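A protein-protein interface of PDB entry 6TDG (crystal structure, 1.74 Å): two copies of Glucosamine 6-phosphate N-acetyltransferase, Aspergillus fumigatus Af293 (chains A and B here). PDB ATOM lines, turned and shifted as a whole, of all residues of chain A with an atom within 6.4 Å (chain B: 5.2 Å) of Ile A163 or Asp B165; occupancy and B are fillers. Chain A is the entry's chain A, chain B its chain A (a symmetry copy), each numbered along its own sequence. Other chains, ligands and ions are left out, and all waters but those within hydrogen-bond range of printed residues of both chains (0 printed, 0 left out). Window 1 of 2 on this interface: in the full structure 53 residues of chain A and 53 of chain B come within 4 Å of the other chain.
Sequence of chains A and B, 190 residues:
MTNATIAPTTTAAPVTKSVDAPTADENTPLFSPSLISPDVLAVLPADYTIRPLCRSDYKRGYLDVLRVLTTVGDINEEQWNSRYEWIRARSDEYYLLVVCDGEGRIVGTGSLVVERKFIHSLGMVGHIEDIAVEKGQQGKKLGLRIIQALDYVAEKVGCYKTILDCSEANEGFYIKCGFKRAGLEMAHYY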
ATOM      1  N   LEU A 112     -13.386 -11.128 -18.461  1.00  0.00           N
ATOM      2  CA  LEU A 112     -13.904  -9.776 -18.252  1.00  0.00           C
ATOM      3  C   LEU A 112     -14.221  -9.587 -16.780  1.00  0.00           C
ATOM      4  O   LEU A 112     -14.975 -10.378 -16.185  1.00  0.00           O
ATOM      5  CB  LEU A 112     -15.144  -9.523 -19.094  1.00  0.00           C
ATOM      6  CG  LEU A 112     -15.698  -8.103 -18.974  1.00  0.00           C
ATOM      7  CD1 LEU A 112     -14.867  -7.198 -19.882  1.00  0.00           C
ATOM      8  CD2 LEU A 112     -17.170  -8.089 -19.352  1.00  0.00           C
ATOM      9  N   GLU A 115     -15.881  -3.632 -13.073  1.00  0.00           N
ATOM     10  CA  GLU A 115     -15.568  -2.740 -11.940  1.00  0.00           C
ATOM     11  C   GLU A 115     -16.735  -1.779 -11.781  1.00  0.00           C
ATOM     12  O   GLU A 115     -17.163  -1.222 -12.787  1.00  0.00           O
ATOM     13  CB  GLU A 115     -14.355  -1.889 -12.276  1.00  0.00           C
ATOM     14  CG  GLU A 115     -13.948  -0.909 -11.189  1.00  0.00           C
ATOM     15  CD  GLU A 115     -13.002   0.165 -11.681  1.00  0.00           C
ATOM     16  OE1 GLU A 115     -12.685   0.148 -12.888  1.00  0.00           O
ATOM     17  OE2 GLU A 115     -12.645   1.046 -10.862  1.00  0.00           O
ATOM     18  N   VAL A 125     -16.984  -0.214 -15.583  1.00  0.00           N
ATOM     19  CA  VAL A 125     -15.896  -0.385 -16.588  1.00  0.00           C
ATOM     20  C   VAL A 125     -15.585  -1.880 -16.731  1.00  0.00           C
ATOM     21  O   VAL A 125     -15.406  -2.548 -15.704  1.00  0.00           O
ATOM     22  CB  VAL A 125     -14.663   0.413 -16.161  1.00  0.00           C
ATOM     23  CG1 VAL A 125     -13.488   0.146 -17.090  1.00  0.00           C
ATOM     24  CG2 VAL A 125     -15.013   1.894 -16.079  1.00  0.00           C
ATOM     25  N   GLY A 126     -15.570  -2.371 -17.967  1.00  0.00           N
ATOM     26  CA  GLY A 126     -15.110  -3.737 -18.272  1.00  0.00           C
ATOM     27  C   GLY A 126     -13.599  -3.779 -18.375  1.00  0.00           C
ATOM     28  O   GLY A 126     -13.008  -2.916 -19.058  1.00  0.00           O
ATOM     29  N   HIS A 127     -12.967  -4.707 -17.679  1.00  0.00           N
ATOM     30  CA  HIS A 127     -11.505  -4.940 -17.736  1.00  0.00           C
ATOM     31  C   HIS A 127     -11.261  -6.303 -18.367  1.00  0.00           C
ATOM     32  O   HIS A 127     -11.631  -7.353 -17.769  1.00  0.00           O
ATOM     33  CB  HIS A 127     -10.907  -4.887 -16.344  1.00  0.00           C
ATOM     34  CG  HIS A 127     -11.114  -3.550 -15.740  1.00  0.00           C
ATOM     35  ND1 HIS A 127     -10.255  -2.492 -15.995  1.00  0.00           N
ATOM     36  CD2 HIS A 127     -12.059  -3.094 -14.876  1.00  0.00           C
ATOM     37  CE1 HIS A 127     -10.678  -1.431 -15.302  1.00  0.00           C
ATOM     38  NE2 HIS A 127     -11.787  -1.781 -14.611  1.00  0.00           N
ATOM     39  N   ILE A 128     -10.577  -6.276 -19.489  1.00  0.00           N
ATOM     40  CA  ILE A 128     -10.231  -7.520 -20.205  1.00  0.00           C
ATOM     41  C   ILE A 128      -8.903  -8.021 -19.642  1.00  0.00           C
ATOM     42  O   ILE A 128      -7.893  -7.221 -19.578  1.00  0.00           O
ATOM     43  CB  ILE A 128     -10.230  -7.272 -21.698  1.00  0.00           C
ATOM     44  CG1 ILE A 128     -11.659  -7.254 -22.224  1.00  0.00           C
ATOM     45  CG2 ILE A 128      -9.375  -8.308 -22.399  1.00  0.00           C
ATOM     46  CD1 ILE A 128     -11.703  -7.154 -23.686  1.00  0.00           C
ATOM     47  N   GLU A 129      -8.870  -9.272 -19.230  1.00  0.00           N
ATOM     48  CA  GLU A 129      -7.698  -9.839 -18.539  1.00  0.00           C
ATOM     49  C   GLU A 129      -7.398 -11.256 -19.015  1.00  0.00           C
ATOM     50  O   GLU A 129      -8.334 -12.013 -19.392  1.00  0.00           O
ATOM     51  CB  GLU A 129      -7.883  -9.876 -17.020  1.00  0.00           C
ATOM     52  CG  GLU A 129      -8.257  -8.536 -16.426  1.00  0.00           C
ATOM     53  CD  GLU A 129      -7.092  -7.579 -16.266  1.00  0.00           C
ATOM     54  OE1 GLU A 129      -5.943  -8.072 -16.244  1.00  0.00           O
ATOM     55  OE2 GLU A 129      -7.340  -6.330 -16.200  1.00  0.00           O
ATOM     56  N   LYS A 161     -17.305   1.402 -21.055  1.00  0.00           N
ATOM     57  CA  LYS A 161     -16.127   1.107 -21.895  1.00  0.00           C
ATOM     58  C   LYS A 161     -15.535  -0.213 -21.413  1.00  0.00           C
ATOM     59  O   LYS A 161     -15.838  -0.617 -20.273  1.00  0.00           O
ATOM     60  CB  LYS A 161     -15.061   2.208 -21.815  1.00  0.00           C
ATOM     61  CG  LYS A 161     -14.426   2.400 -20.455  1.00  0.00           C
ATOM     62  CD  LYS A 161     -13.531   3.587 -20.353  1.00  0.00           C
ATOM     63  CE  LYS A 161     -12.885   3.699 -18.985  1.00  0.00           C
ATOM     64  NZ  LYS A 161     -12.002   4.887 -18.900  1.00  0.00           N
ATOM     65  N   THR A 162     -14.681  -0.771 -22.248  1.00  0.00           N
ATOM     66  CA  THR A 162     -13.765  -1.868 -21.873  1.00  0.00           C
ATOM     67  C   THR A 162     -12.333  -1.386 -22.062  1.00  0.00           C
ATOM     68  O   THR A 162     -12.062  -0.716 -23.048  1.00  0.00           O
ATOM     69  CB  THR A 162     -14.028  -3.103 -22.714  1.00  0.00           C
ATOM     70  OG1 THR A 162     -15.337  -3.550 -22.354  1.00  0.00           O
ATOM     71  CG2 THR A 162     -13.016  -4.179 -22.434  1.00  0.00           C
ATOM     72  N   ILE A 163     -11.493  -1.686 -21.100  1.00  0.00           N
ATOM     73  CA  ILE A 163     -10.068  -1.318 -21.174  1.00  0.00           C
ATOM     74  C   ILE A 163      -9.241  -2.559 -20.868  1.00  0.00           C
ATOM     75  O   ILE A 163      -9.715  -3.501 -20.262  1.00  0.00           O
ATOM     76  CB  ILE A 163      -9.749  -0.112 -20.252  1.00  0.00           C
ATOM     77  CG1 ILE A 163     -10.000  -0.379 -18.775  1.00  0.00           C
ATOM     78  CG2 ILE A 163     -10.508   1.163 -20.690  1.00  0.00           C
ATOM     79  CD1 ILE A 163      -9.368   0.685 -17.865  1.00  0.00           C
ATOM     80  N   LEU A 164      -7.982  -2.483 -21.202  1.00  0.00           N
ATOM     81  CA  LEU A 164      -7.010  -3.541 -20.895  1.00  0.00           C
ATOM     82  C   LEU A 164      -5.649  -2.881 -20.977  1.00  0.00           C
ATOM     83  O   LEU A 164      -5.551  -1.794 -21.594  1.00  0.00           O
ATOM     84  CB  LEU A 164      -7.159  -4.688 -21.905  1.00  0.00           C
ATOM     85  CG  LEU A 164      -6.965  -4.350 -23.387  1.00  0.00           C
ATOM     86  CD1 LEU A 164      -5.509  -4.432 -23.865  1.00  0.00           C
ATOM     87  CD2 LEU A 164      -7.819  -5.259 -24.243  1.00  0.00           C
ATOM     88  N   ASP A 165      -4.670  -3.551 -20.400  1.00  0.00           N
ATOM     89  CA  ASP A 165      -3.243  -3.221 -20.526  1.00  0.00           C
ATOM     90  C   ASP A 165      -2.581  -4.270 -21.423  1.00  0.00           C
ATOM     91  O   ASP A 165      -2.877  -5.478 -21.270  1.00  0.00           O
ATOM     92  CB  ASP A 165      -2.632  -3.165 -19.147  1.00  0.00           C
ATOM     93  CG  ASP A 165      -3.185  -2.083 -18.235  1.00  0.00           C
ATOM     94  OD1 ASP A 165      -3.365  -0.943 -18.696  1.00  0.00           O
ATOM     95  OD2 ASP A 165      -3.375  -2.387 -17.074  1.00  0.00           O
ATOM     96  N   PHE A 179      -9.341  -1.921 -30.584  1.00  0.00           N
ATOM     97  CA  PHE A 179      -8.954  -1.090 -29.408  1.00  0.00           C
ATOM     98  C   PHE A 179      -8.019   0.037 -29.860  1.00  0.00           C
ATOM     99  O   PHE A 179      -7.300  -0.157 -30.846  1.00  0.00           O
ATOM    100  CB  PHE A 179      -8.312  -1.926 -28.305  1.00  0.00           C
ATOM    101  CG  PHE A 179      -9.284  -2.730 -27.492  1.00  0.00           C
ATOM    102  CD1 PHE A 179     -10.022  -3.749 -28.084  1.00  0.00           C
ATOM    103  CD2 PHE A 179      -9.519  -2.427 -26.153  1.00  0.00           C
ATOM    104  CE1 PHE A 179     -10.959  -4.455 -27.343  1.00  0.00           C
ATOM    105  CE2 PHE A 179     -10.458  -3.131 -25.416  1.00  0.00           C
ATOM    106  CZ  PHE A 179     -11.164  -4.155 -26.013  1.00  0.00           C
ATOM    107  N   ALA A 182      -5.067   4.556 -25.065  1.00  0.00           N
ATOM    108  CA  ALA A 182      -5.856   5.493 -24.217  1.00  0.00           C
ATOM    109  C   ALA A 182      -5.026   6.038 -23.064  1.00  0.00           C
ATOM    110  O   ALA A 182      -5.499   6.943 -22.396  1.00  0.00           O
ATOM    111  CB  ALA A 182      -7.084   4.826 -23.692  1.00  0.00           C
ATOM    112  N   GLY A 183      -3.877   5.452 -22.771  1.00  0.00           N
ATOM    113  CA  GLY A 183      -3.005   5.974 -21.716  1.00  0.00           C
ATOM    114  C   GLY A 183      -1.906   4.999 -21.423  1.00  0.00           C
ATOM    115  O   GLY A 183      -1.585   4.189 -22.288  1.00  0.00           O
ATOM    116  N   LEU A 184      -1.335   5.099 -20.240  1.00  0.00           N
ATOM    117  CA  LEU A 184      -0.132   4.341 -19.855  1.00  0.00           C
ATOM    118  C   LEU A 184      -0.510   3.462 -18.675  1.00  0.00           C
ATOM    119  O   LEU A 184      -1.284   3.921 -17.816  1.00  0.00           O
ATOM    120  CB  LEU A 184       0.990   5.281 -19.427  1.00  0.00           C
ATOM    121  CG  LEU A 184       1.449   6.269 -20.488  1.00  0.00           C
ATOM    122  CD1 LEU A 184       2.357   7.331 -19.877  1.00  0.00           C
ATOM    123  CD2 LEU A 184       2.143   5.542 -21.629  1.00  0.00           C
ATOM    124  N   GLU A 185       0.077   2.275 -18.636  1.00  0.00           N
ATOM    125  CA  GLU A 185       0.017   1.369 -17.485  1.00  0.00           C
ATOM    126  C   GLU A 185       1.245   1.637 -16.627  1.00  0.00           C
ATOM    127  O   GLU A 185       2.358   1.642 -17.137  1.00  0.00           O
ATOM    128  CB  GLU A 185      -0.084  -0.085 -17.923  1.00  0.00           C
ATOM    129  CG  GLU A 185      -0.046  -1.027 -16.736  1.00  0.00           C
ATOM    130  CD  GLU A 185       0.264  -2.490 -16.971  1.00  0.00           C
ATOM    131  OE1 GLU A 185       0.644  -2.865 -18.115  1.00  0.00           O
ATOM    132  OE2 GLU A 185       0.178  -3.224 -15.964  1.00  0.00           O
ATOM    133  N   MET A 186       1.032   1.911 -15.347  1.00  0.00           N
ATOM    134  CA  MET A 186       2.107   2.166 -14.375  1.00  0.00           C
ATOM    135  C   MET A 186       2.033   1.051 -13.339  1.00  0.00           C
ATOM    136  O   MET A 186       0.901   0.570 -12.999  1.00  0.00           O
ATOM    137  CB  MET A 186       1.925   3.526 -13.692  1.00  0.00           C
ATOM    138  CG  MET A 186       1.776   4.678 -14.648  1.00  0.00           C
ATOM    139  SD  MET A 186       3.298   4.993 -15.610  1.00  0.00           S
ATOM    140  CE  MET A 186       4.370   5.580 -14.304  1.00  0.00           C
ATOM    141  N   ILE B 128      -5.279   0.609  -8.606  1.00  0.00           N
ATOM    142  CA  ILE B 128      -5.486   1.947  -8.017  1.00  0.00           C
ATOM    143  C   ILE B 128      -6.402   2.727  -8.957  1.00  0.00           C
ATOM    144  O   ILE B 128      -6.112   2.808 -10.212  1.00  0.00           O
ATOM    145  CB  ILE B 128      -4.149   2.605  -7.749  1.00  0.00           C
ATOM    146  CG1 ILE B 128      -3.536   2.035  -6.477  1.00  0.00           C
ATOM    147  CG2 ILE B 128      -4.312   4.110  -7.681  1.00  0.00           C
ATOM    148  CD1 ILE B 128      -2.305   2.739  -6.101  1.00  0.00           C
ATOM    149  N   ILE B 163      -1.169  -1.818  -9.919  1.00  0.00           N
ATOM    150  CA  ILE B 163      -1.077  -1.159 -11.233  1.00  0.00           C
ATOM    151  C   ILE B 163      -2.159  -0.090 -11.305  1.00  0.00           C
ATOM    152  O   ILE B 163      -3.137  -0.131 -10.583  1.00  0.00           O
ATOM    153  CB  ILE B 163      -1.142  -2.192 -12.388  1.00  0.00           C
ATOM    154  CG1 ILE B 163      -2.444  -2.978 -12.443  1.00  0.00           C
ATOM    155  CG2 ILE B 163       0.057  -3.169 -12.353  1.00  0.00           C
ATOM    156  CD1 ILE B 163      -2.624  -3.735 -13.767  1.00  0.00           C
ATOM    157  N   LEU B 164      -2.011   0.787 -12.260  1.00  0.00           N
ATOM    158  CA  LEU B 164      -3.005   1.830 -12.547  1.00  0.00           C
ATOM    159  C   LEU B 164      -2.726   2.280 -13.966  1.00  0.00           C
ATOM    160  O   LEU B 164      -1.605   2.019 -14.464  1.00  0.00           O
ATOM    161  CB  LEU B 164      -2.857   2.976 -11.536  1.00  0.00           C
ATOM    162  CG  LEU B 164      -1.502   3.688 -11.472  1.00  0.00           C
ATOM    163  CD1 LEU B 164      -1.357   4.853 -12.459  1.00  0.00           C
ATOM    164  CD2 LEU B 164      -1.245   4.191 -10.069  1.00  0.00           C
ATOM    165  N   ASP B 165      -3.708   2.949 -14.540  1.00  0.00           N
ATOM    166  CA  ASP B 165      -3.597   3.660 -15.822  1.00  0.00           C
ATOM    167  C   ASP B 165      -3.586   5.164 -15.541  1.00  0.00           C
ATOM    168  O   ASP B 165      -4.383   5.633 -14.694  1.00  0.00           O
ATOM    169  CB  ASP B 165      -4.742   3.243 -16.712  1.00  0.00           C
ATOM    170  CG  ASP B 165      -4.760   1.774 -17.101  1.00  0.00           C
ATOM    171  OD1 ASP B 165      -3.696   1.232 -17.450  1.00  0.00           O
ATOM    172  OD2 ASP B 165      -5.840   1.217 -17.100  1.00  0.00           O
ATOM    173  N   CYS B 166      -2.767   5.893 -16.284  1.00  0.00           N
ATOM    174  CA  CYS B 166      -2.676   7.359 -16.198  1.00  0.00           C
ATOM    175  C   CYS B 166      -2.518   7.958 -17.578  1.00  0.00           C
ATOM    176  O   CYS B 166      -2.408   7.233 -18.539  1.00  0.00           O
ATOM    177  CB  CYS B 166      -1.547   7.786 -15.264  1.00  0.00           C
ATOM    178  SG  CYS B 166       0.100   7.452 -15.879  1.00  0.00           S
ATOM    179  N   SER B 167      -2.529   9.282 -17.642  1.00  0.00           N
ATOM    180  CA  SER B 167      -2.326  10.060 -18.886  1.00  0.00           C
ATOM    181  C   SER B 167      -0.850  10.380 -18.984  1.00  0.00           C
ATOM    182  O   SER B 167      -0.163  10.307 -17.966  1.00  0.00           O
ATOM    183  CB  SER B 167      -3.137  11.339 -18.854  1.00  0.00           C
ATOM    184  OG  SER B 167      -2.704  12.148 -17.765  1.00  0.00           O
ATOM    185  N   GLU B 185      -2.291   1.297 -21.947  1.00  0.00           N
ATOM    186  CA  GLU B 185      -3.736   1.185 -21.721  1.00  0.00           C
ATOM    187  C   GLU B 185      -4.420   1.285 -23.076  1.00  0.00           C
ATOM    188  O   GLU B 185      -4.154   2.213 -23.828  1.00  0.00           O
ATOM    189  CB  GLU B 185      -4.231   2.235 -20.737  1.00  0.00           C
ATOM    190  CG  GLU B 185      -5.738   2.182 -20.579  1.00  0.00           C
ATOM    191  CD  GLU B 185      -6.453   3.370 -19.973  1.00  0.00           C
ATOM    192  OE1 GLU B 185      -5.811   4.437 -19.764  1.00  0.00           O
ATOM    193  OE2 GLU B 185      -7.678   3.217 -19.781  1.00  0.00           O
ATOM    194  N   MET B 186      -5.251   0.303 -23.400  1.00  0.00           N
ATOM    195  CA  MET B 186      -6.014   0.259 -24.658  1.00  0.00           C
ATOM    196  C   MET B 186      -7.488   0.326 -24.277  1.00  0.00           C
ATOM    197  O   MET B 186      -7.896  -0.236 -23.207  1.00  0.00           O
ATOM    198  CB  MET B 186      -5.733  -1.033 -25.432  1.00  0.00           C
ATOM    199  CG  MET B 186      -4.272  -1.297 -25.676  1.00  0.00           C
ATOM    200  SD  MET B 186      -3.516  -0.070 -26.800  1.00  0.00           S
ATOM    201  CE  MET B 186      -4.349  -0.495 -28.324  1.00  0.00           C
ATOM    202  N   ALA B 187      -8.305   0.951 -25.103  1.00  0.00           N
ATOM    203  CA  ALA B 187      -9.716   1.174 -24.749  1.00  0.00           C
ATOM    204  C   ALA B 187     -10.602   0.851 -25.936  1.00  0.00           C
ATOM    205  O   ALA B 187     -10.201   1.110 -27.104  1.00  0.00           O
ATOM    206  CB  ALA B 187      -9.972   2.598 -24.264  1.00  0.00           C
ATOM    207  N   HIS B 188     -11.816   0.407 -25.616  1.00  0.00           N
ATOM    208  CA  HIS B 188     -12.912   0.190 -26.606  1.00  0.00           C
ATOM    209  C   HIS B 188     -14.197   0.798 -26.034  1.00  0.00           C
ATOM    210  O   HIS B 188     -14.559   0.414 -24.924  1.00  0.00           O
ATOM    211  CB  HIS B 188     -13.026  -1.317 -26.857  1.00  0.00           C
ATOM    212  CG  HIS B 188     -13.957  -1.709 -27.945  1.00  0.00           C
ATOM    213  ND1 HIS B 188     -15.301  -1.930 -27.716  1.00  0.00           N
ATOM    214  CD2 HIS B 188     -13.742  -1.949 -29.259  1.00  0.00           C
ATOM    215  CE1 HIS B 188     -15.892  -2.248 -28.855  1.00  0.00           C
ATOM    216  NE2 HIS B 188     -14.953  -2.269 -29.819  1.00  0.00           N
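O of Thr A162 sits at hydrogen-bond distance from N of His B188 (2.8 Å).
The backbone NH of Met A186 lies within hydrogen-bond range of the backbone carbonyl oxygen of Leu B164 (2.8 Å).
N of Ala A182 sits at hydrogen-bond distance from O of Glu B185 (2.8 Å).
The backbone carbonyl oxygen (O) of Leu A164 lies within hydrogen-bond range of the backbone NH (N) of Met B186, 2.8 Å away.
The side-chain carboxylate (OD1) of Asp B165 sits close to the side-chain carboxylate (OD1) of Asp A165, 2.5 Å away.
The backbone carbonyl oxygen (O) of Gly A183 sits at hydrogen-bond distance from the backbone NH (N) of Glu B185 (3.0 Å).
O of Leu A184 sits at hydrogen-bond distance from N of Cys B166 (2.9 Å).
Ile A163 touches Asp B165, and with the chains exchanged Asp A165 touches Ile B163.
Ile A163 touches Glu B185, and with the chains exchanged Glu A185 touches Ile B163.
Leu A164 touches Met B186, and with the chains exchanged Met A186 touches Leu B164.
Asp A165 touches its own counterpart, Asp B165.
Positions printed for both chains: 128, 163, 164, 165, 185 and 186.
Of the 28 pairs that touch across the chains among the printed residues, 13 have their exchanged pair printed and touching as well.
The backbone NH of Ile B128 sits at hydrogen-bond distance from the backbone carbonyl oxygen of Ile B163 (3.0 Å).
The backbone NH (N) of Gly A126 sits at hydrogen-bond distance from the backbone carbonyl oxygen (O) of Lys A161 (2.9 Å).
The backbone NH (N) of Ile A128 is in hydrogen-bond range of the backbone carbonyl oxygen (O) of Ile A163 (3.0 Å).
The backbone NH (N) of Ile A163 is in hydrogen-bond range of the backbone carbonyl oxygen (O) of Gly A126, at 2.8 Å.
Hydrophobic or aromatic side chains of chain A that line the printed part of chain B: Ile A163, Leu A164, Phe A179, Ala A182 and Met A186.
Along chain A the printed residues that touch a printed residue of chain B span positions 161 to 186.
Of the 10 printed residues of chain B, 8 touch a printed residue of chain A.
Printed residues of chain B that touch a printed residue of chain A: Ile B163, Leu B164, Asp B165, Cys B166, Glu B185, Met B186, Ala B187 and His B188.
Hydrophobic or aromatic side chains of chain B that line the printed part of chain A: Ile B163, Leu B164, Met B186, Ala B187 and His B188.
Leu A112 touches none of the printed residues of chain B.
Glu A115 touches none of the printed residues of chain B.
Printed residues of chain B within 4 Å of Thr A162: Ala B187 (3.5 Å) and His B188 (2.8 Å).
Of chain B, only Asp B165 (3.6 Å), Glu B185 (3.6 Å), Met B186 (3.2 Å) and Ala B187 (3.9 Å) come within 4 Å of Ile A163.
Asp B165 touches four residues of chain A.
Of the printed residues of chain A, His B188 touches Lys A161 (3.5 Å), Thr A162 (2.8 Å) and Phe A179 (3.5 Å).
The nearest residue of chain B that does not touch Ile A163 is His B188 (5.0 Å).
The nearest residue of chain A that does not touch Asp B165 is Met A186 (4.9 Å).
Lys A161 touches His B188.
Ile A163 touches Asp B165 (CD1 to OD2, 3.6 Å).
Glu B185 touches Ile A163.
Ile A163 touches Ala B187.
Phe A179 touches Ala B187.
Cys B166 touches Gly A183.
O of Leu B164 touches O of Leu A184, at 3.9 Å.
Ile B163 touches Glu A185 (CD1 to OE2, 3.6 Å).
Asp B165 touches Glu A185.
CG of Met A186 touches SG of Cys B166, at 3.5 Å.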
